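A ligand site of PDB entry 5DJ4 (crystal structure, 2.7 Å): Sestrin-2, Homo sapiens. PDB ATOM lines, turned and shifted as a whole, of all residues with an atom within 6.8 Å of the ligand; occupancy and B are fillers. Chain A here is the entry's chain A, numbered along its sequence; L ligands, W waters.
The side-chain hydroxyl (OG1) of Thr 386 sits at hydrogen-bond distance from an oxygen (O1) of the ligand (2.5 Å). O2 of the ligand lies within hydrogen-bond range of N of Tyr 375, 2.7 Å away. OG1 of Thr 374 sits at hydrogen-bond distance from O1 of the ligand (2.7 Å). N1 of the ligand lies within salt-bridge range of OE2 of Glu 451 (3.0 Å). The backbone carbonyl oxygen of Thr 377 lies close to a nitrogen (N1) of the ligand (3.2 Å). OG1 of Thr 377 is in hydrogen-bond range of N1 of the ligand (3.5 Å). An oxygen (O2) of the ligand sits at hydrogen-bond distance from the backbone NH (N) of Asn 376, at 3.4 Å. O1 of the ligand is in salt-bridge range of NE of Arg 390.
The side-chain hydroxyl of Thr 374 is in hydrogen-bond range of the side-chain hydroxyl of Thr 386 (3.5 Å). The guanidinium group (NE) of Arg 390 lies within hydrogen-bond range of the side-chain hydroxyl (OG1) of Thr 386. N of Asn 376 sits at hydrogen-bond distance from OG1 of Thr 374. The side-chain carboxylate (OE2) of Glu 451 lies within salt-bridge range of the guanidinium group (NH1) of Arg 448 (3.2 Å). The guanidinium group (NH2) of Arg 448 is in hydrogen-bond range of the side-chain hydroxyl (OG1) of Thr 377 (3.2 Å). O of Leu 373 sits at hydrogen-bond distance from NE2 of His 454. The backbone NH (N) of Val 384 sits at hydrogen-bond distance from the backbone carbonyl oxygen (O) of Asn 376 (3.1 Å). The guanidinium group (NH1) of Arg 390 is in hydrogen-bond range of the backbone carbonyl oxygen (O) of Leu 373, at 3.5 Å.
CD2 of His 454 touches C3 of the ligand (3.4 Å). Val 455 touches the ligand (CG2 to C6, 3.98 Å). Hydrophobic or aromatic side chains within 4 Å of the ligand: Tyr 375, His 454 and Val 455. The nearest printed residue that does not touch the ligand is Trp 444 (4.01 Å).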
ATOM      1  N   LEU A 373     -17.660  15.348  -8.137  1.00  0.00           N
ATOM      2  CA  LEU A 373     -16.314  15.571  -7.616  1.00  0.00           C
ATOM      3  C   LEU A 373     -15.265  14.771  -8.384  1.00  0.00           C
ATOM      4  O   LEU A 373     -15.374  13.566  -8.519  1.00  0.00           O
ATOM      5  CB  LEU A 373     -16.271  15.228  -6.126  1.00  0.00           C
ATOM      6  CG  LEU A 373     -14.956  15.415  -5.384  1.00  0.00           C
ATOM      7  CD1 LEU A 373     -14.617  16.869  -5.214  1.00  0.00           C
ATOM      8  CD2 LEU A 373     -15.025  14.738  -4.060  1.00  0.00           C
ATOM      9  N   THR A 374     -14.254  15.470  -8.891  1.00  0.00           N
ATOM     10  CA  THR A 374     -13.166  14.818  -9.613  1.00  0.00           C
ATOM     11  C   THR A 374     -11.935  15.705  -9.701  1.00  0.00           C
ATOM     12  O   THR A 374     -12.042  16.918  -9.736  1.00  0.00           O
ATOM     13  CB  THR A 374     -13.585  14.394 -11.031  1.00  0.00           C
ATOM     14  OG1 THR A 374     -12.487  13.716 -11.662  1.00  0.00           O
ATOM     15  CG2 THR A 374     -13.968  15.573 -11.862  1.00  0.00           C
ATOM     16  N   TYR A 375     -10.764  15.085  -9.726  1.00  0.00           N
ATOM     17  CA  TYR A 375      -9.504  15.775  -9.913  1.00  0.00           C
ATOM     18  C   TYR A 375      -8.894  15.328 -11.223  1.00  0.00           C
ATOM     19  O   TYR A 375      -7.793  15.735 -11.590  1.00  0.00           O
ATOM     20  CB  TYR A 375      -8.568  15.514  -8.745  1.00  0.00           C
ATOM     21  CG  TYR A 375      -9.215  15.831  -7.433  1.00  0.00           C
ATOM     22  CD1 TYR A 375      -9.203  17.125  -6.938  1.00  0.00           C
ATOM     23  CD2 TYR A 375      -9.877  14.859  -6.697  1.00  0.00           C
ATOM     24  CE1 TYR A 375      -9.826  17.439  -5.759  1.00  0.00           C
ATOM     25  CE2 TYR A 375     -10.485  15.154  -5.522  1.00  0.00           C
ATOM     26  CZ  TYR A 375     -10.457  16.448  -5.058  1.00  0.00           C
ATOM     27  OH  TYR A 375     -11.064  16.746  -3.869  1.00  0.00           O
ATOM     28  N   ASN A 376      -9.651  14.498 -11.930  1.00  0.00           N
ATOM     29  CA  ASN A 376      -9.209  13.892 -13.177  1.00  0.00           C
ATOM     30  C   ASN A 376      -7.929  13.105 -12.989  1.00  0.00           C
ATOM     31  O   ASN A 376      -7.073  13.106 -13.857  1.00  0.00           O
ATOM     32  CB  ASN A 376      -9.042  14.961 -14.245  1.00  0.00           C
ATOM     33  CG  ASN A 376     -10.351  15.601 -14.617  1.00  0.00           C
ATOM     34  OD1 ASN A 376     -11.277  14.928 -15.045  1.00  0.00           O
ATOM     35  ND2 ASN A 376     -10.446  16.898 -14.418  1.00  0.00           N
ATOM     36  N   THR A 377      -7.811  12.451 -11.846  1.00  0.00           N
ATOM     37  CA  THR A 377      -6.652  11.631 -11.553  1.00  0.00           C
ATOM     38  C   THR A 377      -7.178  10.245 -11.300  1.00  0.00           C
ATOM     39  O   THR A 377      -8.351  10.082 -11.036  1.00  0.00           O
ATOM     40  CB  THR A 377      -5.854  12.163 -10.336  1.00  0.00           C
ATOM     41  OG1 THR A 377      -6.666  12.098  -9.154  1.00  0.00           O
ATOM     42  CG2 THR A 377      -5.414  13.574 -10.558  1.00  0.00           C
ATOM     43  N   ILE A 378      -6.332   9.232 -11.424  1.00  0.00           N
ATOM     44  CA  ILE A 378      -6.802   7.860 -11.266  1.00  0.00           C
ATOM     45  C   ILE A 378      -5.975   7.064 -10.259  1.00  0.00           C
ATOM     46  O   ILE A 378      -6.508   6.193  -9.599  1.00  0.00           O
ATOM     47  CB  ILE A 378      -6.844   7.137 -12.604  1.00  0.00           C
ATOM     48  CG1 ILE A 378      -8.169   6.387 -12.755  1.00  0.00           C
ATOM     49  CG2 ILE A 378      -5.695   6.189 -12.747  1.00  0.00           C
ATOM     50  CD1 ILE A 378      -8.253   5.159 -11.915  1.00  0.00           C
ATOM     51  N   ALA A 379      -4.698   7.367 -10.133  1.00  0.00           N
ATOM     52  CA  ALA A 379      -3.917   6.878  -9.012  1.00  0.00           C
ATOM     53  C   ALA A 379      -2.609   7.635  -9.036  1.00  0.00           C
ATOM     54  O   ALA A 379      -2.473   8.672  -8.389  1.00  0.00           O
ATOM     55  CB  ALA A 379      -3.679   5.390  -9.097  1.00  0.00           C
ATOM     56  N   VAL A 384      -7.179  12.022 -16.724  1.00  0.00           N
ATOM     57  CA  VAL A 384      -8.145  10.955 -16.948  1.00  0.00           C
ATOM     58  C   VAL A 384      -9.577  11.336 -16.573  1.00  0.00           C
ATOM     59  O   VAL A 384      -9.812  11.796 -15.474  1.00  0.00           O
ATOM     60  CB  VAL A 384      -7.778   9.720 -16.112  1.00  0.00           C
ATOM     61  CG1 VAL A 384      -8.506   8.505 -16.631  1.00  0.00           C
ATOM     62  CG2 VAL A 384      -6.297   9.501 -16.141  1.00  0.00           C
ATOM     63  N   ASP A 385     -10.512  11.154 -17.495  1.00  0.00           N
ATOM     64  CA  ASP A 385     -11.938  11.218 -17.177  1.00  0.00           C
ATOM     65  C   ASP A 385     -12.298   9.971 -16.396  1.00  0.00           C
ATOM     66  O   ASP A 385     -12.135   8.880 -16.891  1.00  0.00           O
ATOM     67  CB  ASP A 385     -12.772  11.317 -18.457  1.00  0.00           C
ATOM     68  CG  ASP A 385     -14.233  11.556 -18.188  1.00  0.00           C
ATOM     69  OD1 ASP A 385     -14.726  11.224 -17.108  1.00  0.00           O
ATOM     70  OD2 ASP A 385     -14.928  12.083 -19.078  1.00  0.00           O
ATOM     71  N   THR A 386     -12.811  10.131 -15.179  1.00  0.00           N
ATOM     72  CA  THR A 386     -13.097   8.991 -14.339  1.00  0.00           C
ATOM     73  C   THR A 386     -14.579   8.752 -14.112  1.00  0.00           C
ATOM     74  O   THR A 386     -14.941   7.955 -13.287  1.00  0.00           O
ATOM     75  CB  THR A 386     -12.447   9.117 -12.966  1.00  0.00           C
ATOM     76  OG1 THR A 386     -12.879  10.335 -12.364  1.00  0.00           O
ATOM     77  CG2 THR A 386     -10.940   9.137 -13.085  1.00  0.00           C
ATOM     78  N   SER A 387     -15.420   9.423 -14.874  1.00  0.00           N
ATOM     79  CA  SER A 387     -16.844   9.411 -14.605  1.00  0.00           C
ATOM     80  C   SER A 387     -17.540   8.063 -14.802  1.00  0.00           C
ATOM     81  O   SER A 387     -18.588   7.839 -14.225  1.00  0.00           O
ATOM     82  CB  SER A 387     -17.520  10.471 -15.442  1.00  0.00           C
ATOM     83  OG  SER A 387     -17.253  10.257 -16.800  1.00  0.00           O
ATOM     84  N   LEU A 389     -16.188   5.250 -13.845  1.00  0.00           N
ATOM     85  CA  LEU A 389     -15.821   4.575 -12.611  1.00  0.00           C
ATOM     86  C   LEU A 389     -16.679   5.047 -11.451  1.00  0.00           C
ATOM     87  O   LEU A 389     -17.163   4.249 -10.673  1.00  0.00           O
ATOM     88  CB  LEU A 389     -14.348   4.837 -12.291  1.00  0.00           C
ATOM     89  CG  LEU A 389     -13.668   4.335 -11.035  1.00  0.00           C
ATOM     90  CD1 LEU A 389     -13.688   2.825 -11.063  1.00  0.00           C
ATOM     91  CD2 LEU A 389     -12.273   4.838 -10.868  1.00  0.00           C
ATOM     92  N   ARG A 390     -16.846   6.356 -11.356  1.00  0.00           N
ATOM     93  CA  ARG A 390     -17.590   6.947 -10.267  1.00  0.00           C
ATOM     94  C   ARG A 390     -19.076   6.677 -10.403  1.00  0.00           C
ATOM     95  O   ARG A 390     -19.778   6.528  -9.409  1.00  0.00           O
ATOM     96  CB  ARG A 390     -17.310   8.447 -10.195  1.00  0.00           C
ATOM     97  CG  ARG A 390     -15.896   8.746  -9.784  1.00  0.00           C
ATOM     98  CD  ARG A 390     -15.604  10.214  -9.699  1.00  0.00           C
ATOM     99  NE  ARG A 390     -15.442  10.824 -11.010  1.00  0.00           N
ATOM    100  CZ  ARG A 390     -16.307  11.665 -11.545  1.00  0.00           C
ATOM    101  NH1 ARG A 390     -17.397  12.017 -10.904  1.00  0.00           N
ATOM    102  NH2 ARG A 390     -16.067  12.170 -12.740  1.00  0.00           N
ATOM    103  N   ILE A 393     -19.674   3.109  -9.089  1.00  0.00           N
ATOM    104  CA  ILE A 393     -19.696   3.065  -7.619  1.00  0.00           C
ATOM    105  C   ILE A 393     -21.049   3.512  -7.091  1.00  0.00           C
ATOM    106  O   ILE A 393     -21.618   2.888  -6.212  1.00  0.00           O
ATOM    107  CB  ILE A 393     -18.598   3.935  -7.010  1.00  0.00           C
ATOM    108  CG1 ILE A 393     -17.229   3.507  -7.543  1.00  0.00           C
ATOM    109  CG2 ILE A 393     -18.660   3.863  -5.509  1.00  0.00           C
ATOM    110  CD1 ILE A 393     -16.080   4.334  -7.089  1.00  0.00           C
ATOM    111  N   TRP A 444      -7.895  -1.638  -3.956  1.00  0.00           N
ATOM    112  CA  TRP A 444      -7.174  -0.553  -4.576  1.00  0.00           C
ATOM    113  C   TRP A 444      -5.812  -0.290  -3.949  1.00  0.00           C
ATOM    114  O   TRP A 444      -5.522   0.802  -3.502  1.00  0.00           O
ATOM    115  CB  TRP A 444      -8.026   0.715  -4.520  1.00  0.00           C
ATOM    116  CG  TRP A 444      -9.133   0.739  -5.513  1.00  0.00           C
ATOM    117  CD1 TRP A 444      -9.515  -0.263  -6.341  1.00  0.00           C
ATOM    118  CD2 TRP A 444      -9.982   1.847  -5.808  1.00  0.00           C
ATOM    119  NE1 TRP A 444     -10.557   0.134  -7.129  1.00  0.00           N
ATOM    120  CE2 TRP A 444     -10.870   1.436  -6.831  1.00  0.00           C
ATOM    121  CE3 TRP A 444     -10.089   3.149  -5.319  1.00  0.00           C
ATOM    122  CZ2 TRP A 444     -11.847   2.275  -7.355  1.00  0.00           C
ATOM    123  CZ3 TRP A 444     -11.064   3.983  -5.835  1.00  0.00           C
ATOM    124  CH2 TRP A 444     -11.921   3.546  -6.848  1.00  0.00           C
ATOM    125  N   PHE A 447      -3.860   2.835  -5.074  1.00  0.00           N
ATOM    126  CA  PHE A 447      -4.535   4.118  -5.066  1.00  0.00           C
ATOM    127  C   PHE A 447      -4.130   4.934  -3.860  1.00  0.00           C
ATOM    128  O   PHE A 447      -3.601   4.401  -2.896  1.00  0.00           O
ATOM    129  CB  PHE A 447      -6.053   3.949  -5.090  1.00  0.00           C
ATOM    130  CG  PHE A 447      -6.610   3.508  -6.412  1.00  0.00           C
ATOM    131  CD1 PHE A 447      -6.245   2.303  -6.960  1.00  0.00           C
ATOM    132  CD2 PHE A 447      -7.531   4.294  -7.075  1.00  0.00           C
ATOM    133  CE1 PHE A 447      -6.775   1.899  -8.169  1.00  0.00           C
ATOM    134  CE2 PHE A 447      -8.069   3.888  -8.283  1.00  0.00           C
ATOM    135  CZ  PHE A 447      -7.687   2.695  -8.828  1.00  0.00           C
ATOM    136  N   ARG A 448      -4.391   6.230  -3.929  1.00  0.00           N
ATOM    137  CA  ARG A 448      -4.080   7.138  -2.842  1.00  0.00           C
ATOM    138  C   ARG A 448      -5.155   7.048  -1.776  1.00  0.00           C
ATOM    139  O   ARG A 448      -6.284   6.665  -2.050  1.00  0.00           O
ATOM    140  CB  ARG A 448      -3.939   8.553  -3.371  1.00  0.00           C
ATOM    141  CG  ARG A 448      -2.604   8.874  -4.016  1.00  0.00           C
ATOM    142  CD  ARG A 448      -2.767   9.592  -5.350  1.00  0.00           C
ATOM    143  NE  ARG A 448      -3.818  10.617  -5.312  1.00  0.00           N
ATOM    144  CZ  ARG A 448      -4.694  10.841  -6.288  1.00  0.00           C
ATOM    145  NH1 ARG A 448      -4.664  10.101  -7.390  1.00  0.00           N
ATOM    146  NH2 ARG A 448      -5.608  11.796  -6.168  1.00  0.00           N
ATOM    147  N   SER A 450      -6.652   9.447  -0.304  1.00  0.00           N
ATOM    148  CA  SER A 450      -7.645  10.462  -0.537  1.00  0.00           C
ATOM    149  C   SER A 450      -8.707   9.934  -1.469  1.00  0.00           C
ATOM    150  O   SER A 450      -9.853  10.364  -1.413  1.00  0.00           O
ATOM    151  CB  SER A 450      -7.006  11.708  -1.126  1.00  0.00           C
ATOM    152  OG  SER A 450      -7.200  11.738  -2.523  1.00  0.00           O
ATOM    153  N   GLU A 451      -8.326   8.998  -2.329  1.00  0.00           N
ATOM    154  CA  GLU A 451      -9.260   8.415  -3.276  1.00  0.00           C
ATOM    155  C   GLU A 451     -10.138   7.398  -2.598  1.00  0.00           C
ATOM    156  O   GLU A 451     -11.242   7.143  -3.032  1.00  0.00           O
ATOM    157  CB  GLU A 451      -8.512   7.775  -4.434  1.00  0.00           C
ATOM    158  CG  GLU A 451      -7.708   8.761  -5.244  1.00  0.00           C
ATOM    159  CD  GLU A 451      -6.918   8.105  -6.352  1.00  0.00           C
ATOM    160  OE1 GLU A 451      -5.921   7.417  -6.058  1.00  0.00           O
ATOM    161  OE2 GLU A 451      -7.286   8.282  -7.524  1.00  0.00           O
ATOM    162  N   LYS A 452      -9.644   6.833  -1.507  1.00  0.00           N
ATOM    163  CA  LYS A 452     -10.430   5.946  -0.676  1.00  0.00           C
ATOM    164  C   LYS A 452     -11.475   6.741   0.099  1.00  0.00           C
ATOM    165  O   LYS A 452     -12.615   6.312   0.242  1.00  0.00           O
ATOM    166  CB  LYS A 452      -9.554   5.190   0.304  1.00  0.00           C
ATOM    167  CG  LYS A 452      -9.343   3.735  -0.047  1.00  0.00           C
ATOM    168  CD  LYS A 452      -8.089   3.511  -0.831  1.00  0.00           C
ATOM    169  CE  LYS A 452      -7.203   2.537  -0.118  1.00  0.00           C
ATOM    170  NZ  LYS A 452      -7.456   1.155  -0.492  1.00  0.00           N
ATOM    171  N   HIS A 454     -12.668   9.534  -0.948  1.00  0.00           N
ATOM    172  CA  HIS A 454     -13.527   9.935  -2.050  1.00  0.00           C
ATOM    173  C   HIS A 454     -14.599   8.889  -2.314  1.00  0.00           C
ATOM    174  O   HIS A 454     -15.746   9.218  -2.519  1.00  0.00           O
ATOM    175  CB  HIS A 454     -12.647  10.183  -3.285  1.00  0.00           C
ATOM    176  CG  HIS A 454     -13.344  10.839  -4.449  1.00  0.00           C
ATOM    177  ND1 HIS A 454     -14.697  10.720  -4.679  1.00  0.00           N
ATOM    178  CD2 HIS A 454     -12.860  11.587  -5.455  1.00  0.00           C
ATOM    179  CE1 HIS A 454     -15.009  11.383  -5.777  1.00  0.00           C
ATOM    180  NE2 HIS A 454     -13.919  11.914  -6.270  1.00  0.00           N
ATOM    181  N   VAL A 455     -14.215   7.616  -2.283  1.00  0.00           N
ATOM    182  CA  VAL A 455     -15.158   6.514  -2.488  1.00  0.00           C
ATOM    183  C   VAL A 455     -16.197   6.510  -1.378  1.00  0.00           C
ATOM    184  O   VAL A 455     -17.376   6.257  -1.602  1.00  0.00           O
ATOM    185  CB  VAL A 455     -14.426   5.150  -2.542  1.00  0.00           C
ATOM    186  CG1 VAL A 455     -15.353   4.000  -2.303  1.00  0.00           C
ATOM    187  CG2 VAL A 455     -13.709   4.997  -3.858  1.00  0.00           C
ATOM    188  N   LEU A 458     -18.852   9.283  -2.013  1.00  0.00           N
ATOM    189  CA  LEU A 458     -19.754   8.832  -3.070  1.00  0.00           C
ATOM    190  C   LEU A 458     -20.782   7.864  -2.534  1.00  0.00           C
ATOM    191  O   LEU A 458     -21.907   7.845  -2.958  1.00  0.00           O
ATOM    192  CB  LEU A 458     -18.937   8.167  -4.157  1.00  0.00           C
ATOM    193  CG  LEU A 458     -17.918   8.856  -5.054  1.00  0.00           C
ATOM    194  CD1 LEU A 458     -17.190   7.900  -5.941  1.00  0.00           C
ATOM    195  CD2 LEU A 458     -18.666   9.892  -5.858  1.00  0.00           C
HETATM  196  N1  LIG L   1      -9.411  10.350  -8.008  1.00  0.00           N
HETATM  197  C1  LIG L   1     -10.608  10.121  -8.802  1.00  0.00           C
HETATM  198  C2  LIG L   1     -11.069  11.402  -9.481  1.00  0.00           C
HETATM  199  O1  LIG L   1     -12.029  11.440 -10.229  1.00  0.00           O
HETATM  200  C3  LIG L   1     -11.728   9.563  -7.923  1.00  0.00           C
HETATM  201  C4  LIG L   1     -11.986   8.061  -7.917  1.00  0.00           C
HETATM  202  C5  LIG L   1     -10.697   7.279  -8.086  1.00  0.00           C
HETATM  203  C6  LIG L   1     -12.700   7.645  -6.648  1.00  0.00           C
HETATM  204  O2  LIG L   1     -10.489  12.443  -9.296  1.00  0.00           O
HETATM  205  O   HOH W   1      -9.815  11.244  -5.541  1.00  0.00           O
